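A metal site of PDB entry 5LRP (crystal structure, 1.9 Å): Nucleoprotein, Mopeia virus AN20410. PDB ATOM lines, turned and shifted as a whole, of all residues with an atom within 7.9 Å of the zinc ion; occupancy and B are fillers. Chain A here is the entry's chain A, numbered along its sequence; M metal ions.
O of His 165 lies close to ND1 of His 146 (3.4 Å).
O of His 68 lies within hydrogen-bond range of ND1 of His 146, at 2.6 Å.
The side-chain carboxylate (OE2) of Glu 36 sits close to a ring nitrogen (NE2) of His 49, at 2.6 Å.
The backbone NH (N) of Ala 167 sits close to the side-chain carboxylate (OE1) of Glu 36, at 3.4 Å.
N of Glu 28 sits at hydrogen-bond distance from O of Glu 36 (2.8 Å).
N of Leu 168 sits close to SG of Cys 166 (3.5 Å).
SG of Cys 166 sits close to N of Leu 169, 3.4 Å away.
The side-chain sulfur of Cys 143 lies close to the backbone NH of Met 145, at 3.8 Å.
His 49 touches the zinc ion.
Of the 23 residues printed, 5 come within 4 Å of the zinc ion.
The zinc ion is bound by NE2 of His 146 (2.0 Å), OE2 of Glu 36 (2.1 Å), SG of Cys 166 (2.3 Å), SG of Cys 143 (2.3 Å) and OE1 of Glu 36 (2.6 Å).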
ATOM      1  N   GLU A  28     -15.871  23.647 -24.017  1.00  0.00           N
ATOM      2  CA  GLU A  28     -14.500  23.792 -24.478  1.00  0.00           C
ATOM      3  C   GLU A  28     -14.476  25.121 -25.226  1.00  0.00           C
ATOM      4  O   GLU A  28     -15.471  25.498 -25.848  1.00  0.00           O
ATOM      5  CB  GLU A  28     -14.100  22.603 -25.355  1.00  0.00           C
ATOM      6  CG  GLU A  28     -14.025  21.281 -24.562  1.00  0.00           C
ATOM      7  CD  GLU A  28     -13.038  21.337 -23.413  1.00  0.00           C
ATOM      8  OE1 GLU A  28     -11.909  21.803 -23.664  1.00  0.00           O
ATOM      9  OE2 GLU A  28     -13.387  20.930 -22.268  1.00  0.00           O
ATOM     10  N   GLU A  36     -17.356  23.675 -28.057  1.00  0.00           N
ATOM     11  CA  GLU A  36     -18.084  22.455 -27.717  1.00  0.00           C
ATOM     12  C   GLU A  36     -18.804  22.615 -26.386  1.00  0.00           C
ATOM     13  O   GLU A  36     -18.220  23.028 -25.394  1.00  0.00           O
ATOM     14  CB  GLU A  36     -17.126  21.260 -27.670  1.00  0.00           C
ATOM     15  CG  GLU A  36     -17.817  19.921 -27.432  1.00  0.00           C
ATOM     16  CD  GLU A  36     -16.954  18.751 -27.827  1.00  0.00           C
ATOM     17  OE1 GLU A  36     -15.727  18.797 -27.576  1.00  0.00           O
ATOM     18  OE2 GLU A  36     -17.490  17.770 -28.393  1.00  0.00           O
ATOM     19  N   ILE A  37     -20.094  22.277 -26.377  1.00  0.00           N
ATOM     20  CA  ILE A  37     -20.891  22.375 -25.174  1.00  0.00           C
ATOM     21  C   ILE A  37     -21.617  21.058 -24.924  1.00  0.00           C
ATOM     22  O   ILE A  37     -22.184  20.493 -25.841  1.00  0.00           O
ATOM     23  CB  ILE A  37     -21.919  23.525 -25.293  1.00  0.00           C
ATOM     24  CG1 ILE A  37     -21.181  24.864 -25.360  1.00  0.00           C
ATOM     25  CG2 ILE A  37     -22.879  23.526 -24.114  1.00  0.00           C
ATOM     26  CD1 ILE A  37     -22.123  26.072 -25.343  1.00  0.00           C
ATOM     27  N   ALA A  38     -21.583  20.556 -23.693  1.00  0.00           N
ATOM     28  CA  ALA A  38     -22.324  19.349 -23.325  1.00  0.00           C
ATOM     29  C   ALA A  38     -23.130  19.585 -22.048  1.00  0.00           C
ATOM     30  O   ALA A  38     -22.623  20.140 -21.076  1.00  0.00           O
ATOM     31  CB  ALA A  38     -21.379  18.148 -23.158  1.00  0.00           C
ATOM     32  N   HIS A  49     -25.524  17.855 -26.796  1.00  0.00           N
ATOM     33  CA  HIS A  49     -24.137  18.014 -27.179  1.00  0.00           C
ATOM     34  C   HIS A  49     -24.043  18.608 -28.564  1.00  0.00           C
ATOM     35  O   HIS A  49     -24.616  18.077 -29.503  1.00  0.00           O
ATOM     36  CB  HIS A  49     -23.454  16.657 -27.130  1.00  0.00           C
ATOM     37  CG  HIS A  49     -22.005  16.699 -27.480  1.00  0.00           C
ATOM     38  ND1 HIS A  49     -21.414  15.723 -28.257  1.00  0.00           N
ATOM     39  CD2 HIS A  49     -21.034  17.576 -27.173  1.00  0.00           C
ATOM     40  CE1 HIS A  49     -20.141  16.011 -28.407  1.00  0.00           C
ATOM     41  NE2 HIS A  49     -19.879  17.128 -27.754  1.00  0.00           N
ATOM     42  N   PHE A  50     -23.310  19.720 -28.703  1.00  0.00           N
ATOM     43  CA  PHE A  50     -23.223  20.395 -30.012  1.00  0.00           C
ATOM     44  C   PHE A  50     -21.956  21.224 -30.098  1.00  0.00           C
ATOM     45  O   PHE A  50     -21.181  21.298 -29.148  1.00  0.00           O
ATOM     46  CB  PHE A  50     -24.467  21.261 -30.266  1.00  0.00           C
ATOM     47  CG  PHE A  50     -24.712  22.306 -29.203  1.00  0.00           C
ATOM     48  CD1 PHE A  50     -25.436  21.992 -28.065  1.00  0.00           C
ATOM     49  CD2 PHE A  50     -24.206  23.591 -29.340  1.00  0.00           C
ATOM     50  CE1 PHE A  50     -25.659  22.938 -27.070  1.00  0.00           C
ATOM     51  CE2 PHE A  50     -24.424  24.560 -28.352  1.00  0.00           C
ATOM     52  CZ  PHE A  50     -25.154  24.222 -27.207  1.00  0.00           C
ATOM     53  N   TYR A  51     -21.731  21.852 -31.253  1.00  0.00           N
ATOM     54  CA  TYR A  51     -20.473  22.538 -31.485  1.00  0.00           C
ATOM     55  C   TYR A  51     -20.726  23.949 -32.031  1.00  0.00           C
ATOM     56  O   TYR A  51     -21.841  24.281 -32.401  1.00  0.00           O
ATOM     57  CB  TYR A  51     -19.591  21.764 -32.462  1.00  0.00           C
ATOM     58  CG  TYR A  51     -19.491  20.285 -32.202  1.00  0.00           C
ATOM     59  CD1 TYR A  51     -18.514  19.761 -31.343  1.00  0.00           C
ATOM     60  CD2 TYR A  51     -20.358  19.389 -32.816  1.00  0.00           C
ATOM     61  CE1 TYR A  51     -18.423  18.381 -31.100  1.00  0.00           C
ATOM     62  CE2 TYR A  51     -20.276  18.007 -32.573  1.00  0.00           C
ATOM     63  CZ  TYR A  51     -19.316  17.516 -31.723  1.00  0.00           C
ATOM     64  OH  TYR A  51     -19.246  16.145 -31.509  1.00  0.00           O
ATOM     65  N   HIS A  68      -8.290  20.817 -26.607  1.00  0.00           N
ATOM     66  CA  HIS A  68      -9.334  19.989 -27.200  1.00  0.00           C
ATOM     67  C   HIS A  68      -9.004  19.326 -28.539  1.00  0.00           C
ATOM     68  O   HIS A  68      -9.734  18.434 -28.964  1.00  0.00           O
ATOM     69  CB  HIS A  68     -10.641  20.795 -27.334  1.00  0.00           C
ATOM     70  CG  HIS A  68     -10.515  22.072 -28.091  1.00  0.00           C
ATOM     71  ND1 HIS A  68     -10.074  22.139 -29.402  1.00  0.00           N
ATOM     72  CD2 HIS A  68     -10.798  23.361 -27.758  1.00  0.00           C
ATOM     73  CE1 HIS A  68     -10.091  23.376 -29.830  1.00  0.00           C
ATOM     74  NE2 HIS A  68     -10.534  24.143 -28.831  1.00  0.00           N
ATOM     75  N   ILE A  70      -9.409  20.051 -31.578  1.00  0.00           N
ATOM     76  CA  ILE A  70     -10.348  20.157 -32.680  1.00  0.00           C
ATOM     77  C   ILE A  70      -9.720  20.913 -33.860  1.00  0.00           C
ATOM     78  O   ILE A  70      -9.036  21.918 -33.666  1.00  0.00           O
ATOM     79  CB  ILE A  70     -11.647  20.840 -32.230  1.00  0.00           C
ATOM     80  CG1 ILE A  70     -12.264  20.034 -31.083  1.00  0.00           C
ATOM     81  CG2 ILE A  70     -12.632  20.985 -33.398  1.00  0.00           C
ATOM     82  CD1 ILE A  70     -13.400  20.735 -30.381  1.00  0.00           C
ATOM     83  N   TRP A 136     -13.043   7.037 -22.166  1.00  0.00           N
ATOM     84  CA  TRP A 136     -12.691   7.155 -23.580  1.00  0.00           C
ATOM     85  C   TRP A 136     -12.785   5.816 -24.299  1.00  0.00           C
ATOM     86  O   TRP A 136     -13.238   5.742 -25.438  1.00  0.00           O
ATOM     87  CB  TRP A 136     -11.296   7.755 -23.720  1.00  0.00           C
ATOM     88  CG  TRP A 136     -11.373   9.245 -23.796  1.00  0.00           C
ATOM     89  CD1 TRP A 136     -11.421  10.119 -22.744  1.00  0.00           C
ATOM     90  CD2 TRP A 136     -11.446  10.043 -24.979  1.00  0.00           C
ATOM     91  NE1 TRP A 136     -11.511  11.420 -23.211  1.00  0.00           N
ATOM     92  CE2 TRP A 136     -11.529  11.395 -24.577  1.00  0.00           C
ATOM     93  CE3 TRP A 136     -11.452   9.746 -26.351  1.00  0.00           C
ATOM     94  CZ2 TRP A 136     -11.610  12.453 -25.491  1.00  0.00           C
ATOM     95  CZ3 TRP A 136     -11.532  10.798 -27.258  1.00  0.00           C
ATOM     96  CH2 TRP A 136     -11.602  12.132 -26.820  1.00  0.00           C
ATOM     97  N   LYS A 140     -15.697   6.953 -26.638  1.00  0.00           N
ATOM     98  CA  LYS A 140     -15.058   7.788 -27.651  1.00  0.00           C
ATOM     99  C   LYS A 140     -15.881   7.853 -28.946  1.00  0.00           C
ATOM    100  O   LYS A 140     -15.822   8.843 -29.670  1.00  0.00           O
ATOM    101  CB  LYS A 140     -13.619   7.297 -27.917  1.00  0.00           C
ATOM    102  CG  LYS A 140     -13.133   7.361 -29.346  1.00  0.00           C
ATOM    103  CD  LYS A 140     -11.862   6.523 -29.524  1.00  0.00           C
ATOM    104  CE  LYS A 140     -11.977   5.151 -28.899  1.00  0.00           C
ATOM    105  NZ  LYS A 140     -10.685   4.400 -28.958  1.00  0.00           N
ATOM    106  N   LEU A 142     -18.850   8.473 -29.242  1.00  0.00           N
ATOM    107  CA  LEU A 142     -19.872   9.509 -29.125  1.00  0.00           C
ATOM    108  C   LEU A 142     -19.387  10.894 -29.604  1.00  0.00           C
ATOM    109  O   LEU A 142     -20.206  11.778 -29.865  1.00  0.00           O
ATOM    110  CB  LEU A 142     -20.363   9.624 -27.693  1.00  0.00           C
ATOM    111  CG  LEU A 142     -21.104   8.393 -27.155  1.00  0.00           C
ATOM    112  CD1 LEU A 142     -21.624   8.661 -25.742  1.00  0.00           C
ATOM    113  CD2 LEU A 142     -22.235   8.005 -28.095  1.00  0.00           C
ATOM    114  N   CYS A 143     -18.086  11.081 -29.701  1.00  0.00           N
ATOM    115  CA  CYS A 143     -17.541  12.324 -30.238  1.00  0.00           C
ATOM    116  C   CYS A 143     -16.219  12.077 -30.932  1.00  0.00           C
ATOM    117  O   CYS A 143     -15.236  11.706 -30.303  1.00  0.00           O
ATOM    118  CB  CYS A 143     -17.340  13.378 -29.140  1.00  0.00           C
ATOM    119  SG  CYS A 143     -16.839  15.020 -29.796  1.00  0.00           S
ATOM    120  N   ARG A 144     -16.216  12.296 -32.240  1.00  0.00           N
ATOM    121  CA  ARG A 144     -15.028  12.020 -33.036  1.00  0.00           C
ATOM    122  C   ARG A 144     -14.363  13.318 -33.515  1.00  0.00           C
ATOM    123  O   ARG A 144     -13.621  13.310 -34.488  1.00  0.00           O
ATOM    124  CB  ARG A 144     -15.367  11.109 -34.213  1.00  0.00           C
ATOM    125  CG  ARG A 144     -15.838   9.711 -33.790  1.00  0.00           C
ATOM    126  CD  ARG A 144     -16.296   8.892 -34.987  1.00  0.00           C
ATOM    127  NE  ARG A 144     -15.711   9.356 -36.239  1.00  0.00           N
ATOM    128  CZ  ARG A 144     -16.320   9.300 -37.419  1.00  0.00           C
ATOM    129  NH1 ARG A 144     -17.545   8.805 -37.510  1.00  0.00           N
ATOM    130  NH2 ARG A 144     -15.716   9.751 -38.507  1.00  0.00           N
ATOM    131  N   MET A 145     -14.639  14.417 -32.823  1.00  0.00           N
ATOM    132  CA  MET A 145     -14.173  15.735 -33.251  1.00  0.00           C
ATOM    133  C   MET A 145     -12.773  16.118 -32.770  1.00  0.00           C
ATOM    134  O   MET A 145     -12.227  17.134 -33.188  1.00  0.00           O
ATOM    135  CB  MET A 145     -15.175  16.772 -32.779  1.00  0.00           C
ATOM    136  CG  MET A 145     -16.532  16.609 -33.407  1.00  0.00           C
ATOM    137  SD  MET A 145     -16.605  17.364 -35.056  1.00  0.00           S
ATOM    138  CE  MET A 145     -15.671  18.841 -34.723  1.00  0.00           C
ATOM    139  N   HIS A 146     -12.176  15.296 -31.923  1.00  0.00           N
ATOM    140  CA  HIS A 146     -10.879  15.619 -31.330  1.00  0.00           C
ATOM    141  C   HIS A 146      -9.768  14.834 -32.024  1.00  0.00           C
ATOM    142  O   HIS A 146      -9.358  13.775 -31.573  1.00  0.00           O
ATOM    143  CB  HIS A 146     -10.924  15.377 -29.817  1.00  0.00           C
ATOM    144  CG  HIS A 146     -12.126  16.005 -29.186  1.00  0.00           C
ATOM    145  ND1 HIS A 146     -12.109  17.300 -28.687  1.00  0.00           N
ATOM    146  CD2 HIS A 146     -13.386  15.548 -29.017  1.00  0.00           C
ATOM    147  CE1 HIS A 146     -13.311  17.592 -28.217  1.00  0.00           C
ATOM    148  NE2 HIS A 146     -14.100  16.552 -28.401  1.00  0.00           N
ATOM    149  N   PRO A 164      -7.251  14.428 -25.378  1.00  0.00           N
ATOM    150  CA  PRO A 164      -7.909  15.727 -25.567  1.00  0.00           C
ATOM    151  C   PRO A 164      -9.096  15.878 -24.640  1.00  0.00           C
ATOM    152  O   PRO A 164      -9.720  14.903 -24.253  1.00  0.00           O
ATOM    153  CB  PRO A 164      -8.388  15.674 -27.025  1.00  0.00           C
ATOM    154  CG  PRO A 164      -7.517  14.706 -27.687  1.00  0.00           C
ATOM    155  CD  PRO A 164      -7.169  13.669 -26.630  1.00  0.00           C
ATOM    156  N   HIS A 165      -9.390  17.115 -24.270  1.00  0.00           N
ATOM    157  CA  HIS A 165     -10.585  17.438 -23.525  1.00  0.00           C
ATOM    158  C   HIS A 165     -11.770  17.529 -24.478  1.00  0.00           C
ATOM    159  O   HIS A 165     -11.735  18.269 -25.473  1.00  0.00           O
ATOM    160  CB  HIS A 165     -10.415  18.749 -22.788  1.00  0.00           C
ATOM    161  CG  HIS A 165      -9.387  18.711 -21.706  1.00  0.00           C
ATOM    162  ND1 HIS A 165      -8.311  17.854 -21.720  1.00  0.00           N
ATOM    163  CD2 HIS A 165      -9.233  19.482 -20.603  1.00  0.00           C
ATOM    164  CE1 HIS A 165      -7.565  18.056 -20.647  1.00  0.00           C
ATOM    165  NE2 HIS A 165      -8.116  19.051 -19.954  1.00  0.00           N
ATOM    166  N   CYS A 166     -12.813  16.773 -24.154  1.00  0.00           N
ATOM    167  CA  CYS A 166     -14.067  16.771 -24.881  1.00  0.00           C
ATOM    168  C   CYS A 166     -15.152  17.174 -23.900  1.00  0.00           C
ATOM    169  O   CYS A 166     -15.214  16.612 -22.805  1.00  0.00           O
ATOM    170  CB  CYS A 166     -14.347  15.378 -25.484  1.00  0.00           C
ATOM    171  SG  CYS A 166     -16.069  15.031 -26.020  1.00  0.00           S
ATOM    172  N   ALA A 167     -15.978  18.161 -24.256  1.00  0.00           N
ATOM    173  CA  ALA A 167     -17.023  18.627 -23.333  1.00  0.00           C
ATOM    174  C   ALA A 167     -17.942  17.475 -22.859  1.00  0.00           C
ATOM    175  O   ALA A 167     -18.339  17.413 -21.689  1.00  0.00           O
ATOM    176  CB  ALA A 167     -17.864  19.725 -23.982  1.00  0.00           C
ATOM    177  N   LEU A 168     -18.266  16.554 -23.759  1.00  0.00           N
ATOM    178  CA  LEU A 168     -19.160  15.453 -23.407  1.00  0.00           C
ATOM    179  C   LEU A 168     -18.444  14.438 -22.551  1.00  0.00           C
ATOM    180  O   LEU A 168     -18.933  14.081 -21.475  1.00  0.00           O
ATOM    181  CB  LEU A 168     -19.724  14.762 -24.660  1.00  0.00           C
ATOM    182  CG  LEU A 168     -20.633  13.547 -24.411  1.00  0.00           C
ATOM    183  CD1 LEU A 168     -21.858  13.966 -23.641  1.00  0.00           C
ATOM    184  CD2 LEU A 168     -20.993  12.865 -25.729  1.00  0.00           C
ATOM    185  N   LEU A 169     -17.288  13.966 -22.990  1.00  0.00           N
ATOM    186  CA  LEU A 169     -16.638  12.884 -22.240  1.00  0.00           C
ATOM    187  C   LEU A 169     -16.130  13.380 -20.885  1.00  0.00           C
ATOM    188  O   LEU A 169     -15.991  12.593 -19.961  1.00  0.00           O
ATOM    189  CB  LEU A 169     -15.512  12.250 -23.058  1.00  0.00           C
ATOM    190  CG  LEU A 169     -16.012  11.017 -23.836  1.00  0.00           C
ATOM    191  CD1 LEU A 169     -17.260  11.314 -24.698  1.00  0.00           C
ATOM    192  CD2 LEU A 169     -14.919  10.396 -24.690  1.00  0.00           C
ATOM    193  N   ASP A 170     -15.859  14.683 -20.774  1.00  0.00           N
ATOM    194  CA  ASP A 170     -15.528  15.308 -19.491  1.00  0.00           C
ATOM    195  C   ASP A 170     -16.694  15.190 -18.514  1.00  0.00           C
ATOM    196  O   ASP A 170     -16.493  14.833 -17.366  1.00  0.00           O
ATOM    197  CB  ASP A 170     -15.195  16.796 -19.646  1.00  0.00           C
ATOM    198  CG  ASP A 170     -13.766  17.055 -20.052  1.00  0.00           C
ATOM    199  OD1 ASP A 170     -13.024  16.061 -20.292  1.00  0.00           O
ATOM    200  OD2 ASP A 170     -13.408  18.254 -20.162  1.00  0.00           O
HETATM  201 ZN    ZN M   1     -16.062  16.253 -27.976  1.00  0.00          ZN
